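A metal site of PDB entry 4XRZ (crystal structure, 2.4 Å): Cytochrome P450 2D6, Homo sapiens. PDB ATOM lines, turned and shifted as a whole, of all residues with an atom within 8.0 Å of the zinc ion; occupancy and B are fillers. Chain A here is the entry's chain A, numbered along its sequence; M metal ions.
The backbone carbonyl oxygen (O) of His 236 sits at hydrogen-bond distance from the side-chain hydroxyl (OG1) of Thr 239. The side-chain hydroxyl (OG1) of Thr 168 lies within hydrogen-bond range of the side-chain sulfur (SG) of Cys 169, 3.4 Å away. OE2 of Glu 251 sits at hydrogen-bond distance from N of Arg 247. NE2 of His 236 lies close to O of Cys 169, 3.1 Å away. The side-chain carboxylate (OD1) of Asp 248 lies within hydrogen-bond range of the backbone NH (N) of Thr 250 (3.3 Å).
Residues that only touch the zinc ion: Cys 169. Four residues have an atom within 4 Å of the zinc ion: Cys 169, His 236, Asp 248 and Glu 251. The nearest printed residue that does not touch the zinc ion is Arg 247 (4.5 Å).
OE1 of Glu 251 binds the zinc ion (1.9 Å). The zinc ion is bound by NE2 of His 236, at 2.0 Å. The zinc ion is bound by the side-chain carboxylate (OD2) of Asp 248, at 2.1 Å. The zinc ion has three donor atoms within binding distance.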
ATOM      1  N   ALA A 165      37.470 -19.087  -4.961  1.00  0.00           N
ATOM      2  CA  ALA A 165      36.238 -19.768  -5.339  1.00  0.00           C
ATOM      3  C   ALA A 165      35.073 -18.787  -5.274  1.00  0.00           C
ATOM      4  O   ALA A 165      34.154 -18.834  -6.091  1.00  0.00           O
ATOM      5  CB  ALA A 165      35.977 -20.962  -4.434  1.00  0.00           C
ATOM      6  N   SER A 166      35.124 -17.880  -4.302  1.00  0.00           N
ATOM      7  CA  SER A 166      34.101 -16.864  -4.148  1.00  0.00           C
ATOM      8  C   SER A 166      34.104 -15.881  -5.306  1.00  0.00           C
ATOM      9  O   SER A 166      33.052 -15.375  -5.708  1.00  0.00           O
ATOM     10  CB  SER A 166      34.302 -16.110  -2.823  1.00  0.00           C
ATOM     11  OG  SER A 166      33.312 -15.113  -2.650  1.00  0.00           O
ATOM     12  N   LEU A 167      35.286 -15.607  -5.842  1.00  0.00           N
ATOM     13  CA  LEU A 167      35.437 -14.670  -6.951  1.00  0.00           C
ATOM     14  C   LEU A 167      35.088 -15.321  -8.284  1.00  0.00           C
ATOM     15  O   LEU A 167      34.532 -14.674  -9.172  1.00  0.00           O
ATOM     16  CB  LEU A 167      36.854 -14.115  -6.992  1.00  0.00           C
ATOM     17  CG  LEU A 167      37.206 -13.088  -5.914  1.00  0.00           C
ATOM     18  CD1 LEU A 167      38.696 -12.766  -5.946  1.00  0.00           C
ATOM     19  CD2 LEU A 167      36.378 -11.831  -6.113  1.00  0.00           C
ATOM     20  N   THR A 168      35.427 -16.599  -8.427  1.00  0.00           N
ATOM     21  CA  THR A 168      35.190 -17.305  -9.684  1.00  0.00           C
ATOM     22  C   THR A 168      33.859 -18.063  -9.699  1.00  0.00           C
ATOM     23  O   THR A 168      33.080 -17.926 -10.643  1.00  0.00           O
ATOM     24  CB  THR A 168      36.326 -18.309  -9.983  1.00  0.00           C
ATOM     25  OG1 THR A 168      36.319 -19.356  -9.007  1.00  0.00           O
ATOM     26  CG2 THR A 168      37.675 -17.597  -9.949  1.00  0.00           C
ATOM     27  N   CYS A 169      33.598 -18.850  -8.666  1.00  0.00           N
ATOM     28  CA  CYS A 169      32.416 -19.704  -8.626  1.00  0.00           C
ATOM     29  C   CYS A 169      31.242 -19.029  -7.909  1.00  0.00           C
ATOM     30  O   CYS A 169      30.093 -19.423  -8.062  1.00  0.00           O
ATOM     31  CB  CYS A 169      32.741 -21.044  -7.957  1.00  0.00           C
ATOM     32  SG  CYS A 169      34.125 -21.954  -8.725  1.00  0.00           S
ATOM     33  N   GLY A 170      31.540 -17.980  -7.142  1.00  0.00           N
ATOM     34  CA  GLY A 170      30.515 -17.264  -6.420  1.00  0.00           C
ATOM     35  C   GLY A 170      30.050 -17.972  -5.161  1.00  0.00           C
ATOM     36  O   GLY A 170      28.916 -17.793  -4.708  1.00  0.00           O
ATOM     37  N   ARG A 171      30.931 -18.786  -4.576  1.00  0.00           N
ATOM     38  CA  ARG A 171      30.598 -19.524  -3.372  1.00  0.00           C
ATOM     39  C   ARG A 171      31.833 -19.905  -2.578  1.00  0.00           C
ATOM     40  O   ARG A 171      32.957 -19.841  -3.078  1.00  0.00           O
ATOM     41  CB  ARG A 171      29.796 -20.787  -3.709  1.00  0.00           C
ATOM     42  CG  ARG A 171      30.644 -21.862  -4.395  1.00  0.00           C
ATOM     43  CD  ARG A 171      29.962 -23.219  -4.368  1.00  0.00           C
ATOM     44  NE  ARG A 171      29.787 -23.717  -2.998  1.00  0.00           N
ATOM     45  CZ  ARG A 171      29.239 -24.884  -2.694  1.00  0.00           C
ATOM     46  NH1 ARG A 171      28.796 -25.690  -3.651  1.00  0.00           N
ATOM     47  NH2 ARG A 171      29.127 -25.241  -1.419  1.00  0.00           N
ATOM     48  N   HIS A 236      26.868 -24.688 -11.379  1.00  0.00           N
ATOM     49  CA  HIS A 236      26.881 -23.231 -11.343  1.00  0.00           C
ATOM     50  C   HIS A 236      26.035 -22.646 -12.464  1.00  0.00           C
ATOM     51  O   HIS A 236      25.363 -21.634 -12.278  1.00  0.00           O
ATOM     52  CB  HIS A 236      28.314 -22.715 -11.431  1.00  0.00           C
ATOM     53  CG  HIS A 236      28.457 -21.257 -11.120  1.00  0.00           C
ATOM     54  ND1 HIS A 236      29.609 -20.545 -11.358  1.00  0.00           N
ATOM     55  CD2 HIS A 236      27.576 -20.374 -10.590  1.00  0.00           C
ATOM     56  CE1 HIS A 236      29.441 -19.290 -10.988  1.00  0.00           C
ATOM     57  NE2 HIS A 236      28.213 -19.160 -10.515  1.00  0.00           N
ATOM     58  N   ARG A 237      26.077 -23.296 -13.632  1.00  0.00           N
ATOM     59  CA  ARG A 237      25.287 -22.866 -14.778  1.00  0.00           C
ATOM     60  C   ARG A 237      23.791 -22.857 -14.460  1.00  0.00           C
ATOM     61  O   ARG A 237      23.064 -21.954 -14.869  1.00  0.00           O
ATOM     62  CB  ARG A 237      25.538 -23.777 -15.976  1.00  0.00           C
ATOM     63  CG  ARG A 237      26.595 -23.281 -16.949  1.00  0.00           C
ATOM     64  CD  ARG A 237      26.487 -24.019 -18.278  1.00  0.00           C
ATOM     65  NE  ARG A 237      27.508 -23.595 -19.241  1.00  0.00           N
ATOM     66  CZ  ARG A 237      28.682 -24.194 -19.378  1.00  0.00           C
ATOM     67  NH1 ARG A 237      28.999 -25.234 -18.621  1.00  0.00           N
ATOM     68  NH2 ARG A 237      29.554 -23.750 -20.275  1.00  0.00           N
ATOM     69  N   THR A 239      22.309 -22.421 -11.588  1.00  0.00           N
ATOM     70  CA  THR A 239      21.935 -21.396 -10.620  1.00  0.00           C
ATOM     71  C   THR A 239      22.150 -19.978 -11.134  1.00  0.00           C
ATOM     72  O   THR A 239      21.679 -19.010 -10.531  1.00  0.00           O
ATOM     73  CB  THR A 239      22.706 -21.568  -9.301  1.00  0.00           C
ATOM     74  OG1 THR A 239      24.119 -21.537  -9.570  1.00  0.00           O
ATOM     75  CG2 THR A 239      22.346 -22.880  -8.630  1.00  0.00           C
ATOM     76  N   TRP A 240      22.856 -19.847 -12.253  1.00  0.00           N
ATOM     77  CA  TRP A 240      23.132 -18.542 -12.840  1.00  0.00           C
ATOM     78  C   TRP A 240      21.855 -17.820 -13.240  1.00  0.00           C
ATOM     79  O   TRP A 240      21.015 -18.365 -13.949  1.00  0.00           O
ATOM     80  CB  TRP A 240      24.055 -18.676 -14.054  1.00  0.00           C
ATOM     81  CG  TRP A 240      24.279 -17.376 -14.795  1.00  0.00           C
ATOM     82  CD1 TRP A 240      24.377 -16.129 -14.256  1.00  0.00           C
ATOM     83  CD2 TRP A 240      24.426 -17.223 -16.210  1.00  0.00           C
ATOM     84  NE1 TRP A 240      24.570 -15.204 -15.242  1.00  0.00           N
ATOM     85  CE2 TRP A 240      24.613 -15.847 -16.459  1.00  0.00           C
ATOM     86  CE3 TRP A 240      24.420 -18.099 -17.297  1.00  0.00           C
ATOM     87  CZ2 TRP A 240      24.782 -15.334 -17.739  1.00  0.00           C
ATOM     88  CZ3 TRP A 240      24.599 -17.588 -18.573  1.00  0.00           C
ATOM     89  CH2 TRP A 240      24.776 -16.217 -18.778  1.00  0.00           C
ATOM     90  N   ASP A 241      21.708 -16.585 -12.777  1.00  0.00           N
ATOM     91  CA  ASP A 241      20.591 -15.736 -13.172  1.00  0.00           C
ATOM     92  C   ASP A 241      21.087 -14.622 -14.084  1.00  0.00           C
ATOM     93  O   ASP A 241      21.585 -13.603 -13.619  1.00  0.00           O
ATOM     94  CB  ASP A 241      19.900 -15.150 -11.939  1.00  0.00           C
ATOM     95  CG  ASP A 241      18.640 -14.365 -12.284  1.00  0.00           C
ATOM     96  OD1 ASP A 241      18.115 -13.665 -11.402  1.00  0.00           O
ATOM     97  OD2 ASP A 241      18.180 -14.453 -13.440  1.00  0.00           O
ATOM     98  N   PRO A 245      23.071  -8.705 -12.896  1.00  0.00           N
ATOM     99  CA  PRO A 245      24.496  -8.516 -13.167  1.00  0.00           C
ATOM    100  C   PRO A 245      25.317  -9.678 -12.608  1.00  0.00           C
ATOM    101  O   PRO A 245      24.979 -10.188 -11.541  1.00  0.00           O
ATOM    102  CB  PRO A 245      24.833  -7.212 -12.454  1.00  0.00           C
ATOM    103  CG  PRO A 245      23.535  -6.478 -12.370  1.00  0.00           C
ATOM    104  CD  PRO A 245      22.492  -7.544 -12.189  1.00  0.00           C
ATOM    105  N   PRO A 246      26.373 -10.094 -13.328  1.00  0.00           N
ATOM    106  CA  PRO A 246      27.229 -11.204 -12.901  1.00  0.00           C
ATOM    107  C   PRO A 246      27.716 -11.050 -11.467  1.00  0.00           C
ATOM    108  O   PRO A 246      28.188  -9.987 -11.078  1.00  0.00           O
ATOM    109  CB  PRO A 246      28.405 -11.160 -13.886  1.00  0.00           C
ATOM    110  CG  PRO A 246      28.278  -9.833 -14.602  1.00  0.00           C
ATOM    111  CD  PRO A 246      26.823  -9.515 -14.593  1.00  0.00           C
ATOM    112  N   ARG A 247      27.585 -12.131 -10.692  1.00  0.00           N
ATOM    113  CA  ARG A 247      27.932 -12.112  -9.284  1.00  0.00           C
ATOM    114  C   ARG A 247      29.360 -12.609  -9.072  1.00  0.00           C
ATOM    115  O   ARG A 247      29.922 -12.480  -7.978  1.00  0.00           O
ATOM    116  CB  ARG A 247      26.951 -12.989  -8.501  1.00  0.00           C
ATOM    117  CG  ARG A 247      26.258 -12.284  -7.345  1.00  0.00           C
ATOM    118  CD  ARG A 247      25.363 -13.260  -6.611  1.00  0.00           C
ATOM    119  NE  ARG A 247      26.010 -14.563  -6.492  1.00  0.00           N
ATOM    120  CZ  ARG A 247      26.850 -14.899  -5.522  1.00  0.00           C
ATOM    121  NH1 ARG A 247      27.149 -14.026  -4.570  1.00  0.00           N
ATOM    122  NH2 ARG A 247      27.408 -16.106  -5.519  1.00  0.00           N
ATOM    123  N   ASP A 248      29.937 -13.172 -10.123  1.00  0.00           N
ATOM    124  CA  ASP A 248      31.284 -13.727 -10.065  1.00  0.00           C
ATOM    125  C   ASP A 248      31.873 -13.799 -11.474  1.00  0.00           C
ATOM    126  O   ASP A 248      31.214 -13.428 -12.440  1.00  0.00           O
ATOM    127  CB  ASP A 248      31.259 -15.114  -9.422  1.00  0.00           C
ATOM    128  CG  ASP A 248      30.183 -16.007 -10.013  1.00  0.00           C
ATOM    129  OD1 ASP A 248      30.404 -16.559 -11.106  1.00  0.00           O
ATOM    130  OD2 ASP A 248      29.114 -16.164  -9.371  1.00  0.00           O
ATOM    131  N   LEU A 249      33.111 -14.274 -11.567  1.00  0.00           N
ATOM    132  CA  LEU A 249      33.829 -14.257 -12.842  1.00  0.00           C
ATOM    133  C   LEU A 249      33.253 -15.249 -13.858  1.00  0.00           C
ATOM    134  O   LEU A 249      33.228 -14.975 -15.052  1.00  0.00           O
ATOM    135  CB  LEU A 249      35.317 -14.547 -12.624  1.00  0.00           C
ATOM    136  CG  LEU A 249      36.237 -14.365 -13.829  1.00  0.00           C
ATOM    137  CD1 LEU A 249      37.536 -13.688 -13.431  1.00  0.00           C
ATOM    138  CD2 LEU A 249      36.525 -15.690 -14.533  1.00  0.00           C
ATOM    139  N   THR A 250      32.792 -16.407 -13.377  1.00  0.00           N
ATOM    140  CA  THR A 250      32.232 -17.419 -14.263  1.00  0.00           C
ATOM    141  C   THR A 250      30.965 -16.920 -14.950  1.00  0.00           C
ATOM    142  O   THR A 250      30.766 -17.141 -16.136  1.00  0.00           O
ATOM    143  CB  THR A 250      31.922 -18.720 -13.502  1.00  0.00           C
ATOM    144  OG1 THR A 250      33.133 -19.242 -12.943  1.00  0.00           O
ATOM    145  CG2 THR A 250      31.326 -19.754 -14.437  1.00  0.00           C
ATOM    146  N   GLU A 251      30.105 -16.240 -14.189  1.00  0.00           N
ATOM    147  CA  GLU A 251      28.884 -15.677 -14.739  1.00  0.00           C
ATOM    148  C   GLU A 251      29.195 -14.601 -15.766  1.00  0.00           C
ATOM    149  O   GLU A 251      28.507 -14.481 -16.794  1.00  0.00           O
ATOM    150  CB  GLU A 251      28.002 -15.114 -13.627  1.00  0.00           C
ATOM    151  CG  GLU A 251      27.460 -16.167 -12.671  1.00  0.00           C
ATOM    152  CD  GLU A 251      26.576 -15.572 -11.592  1.00  0.00           C
ATOM    153  OE1 GLU A 251      26.301 -16.275 -10.601  1.00  0.00           O
ATOM    154  OE2 GLU A 251      26.155 -14.408 -11.739  1.00  0.00           O
ATOM    155  N   ALA A 252      30.228 -13.799 -15.495  1.00  0.00           N
ATOM    156  CA  ALA A 252      30.651 -12.751 -16.413  1.00  0.00           C
ATOM    157  C   ALA A 252      31.146 -13.371 -17.713  1.00  0.00           C
ATOM    158  O   ALA A 252      30.872 -12.866 -18.801  1.00  0.00           O
ATOM    159  CB  ALA A 252      31.736 -11.897 -15.779  1.00  0.00           C
ATOM    160  N   LEU A 254      30.242 -16.335 -18.890  1.00  0.00           N
ATOM    161  CA  LEU A 254      29.060 -16.908 -19.540  1.00  0.00           C
ATOM    162  C   LEU A 254      28.272 -15.841 -20.297  1.00  0.00           C
ATOM    163  O   LEU A 254      27.762 -16.092 -21.395  1.00  0.00           O
ATOM    164  CB  LEU A 254      28.164 -17.591 -18.516  1.00  0.00           C
ATOM    165  CG  LEU A 254      28.662 -18.896 -17.902  1.00  0.00           C
ATOM    166  CD1 LEU A 254      27.848 -19.249 -16.665  1.00  0.00           C
ATOM    167  CD2 LEU A 254      28.609 -20.028 -18.914  1.00  0.00           C
HETATM  168 ZN    ZN M   1      27.562 -17.472  -9.754  1.00  0.00          ZN
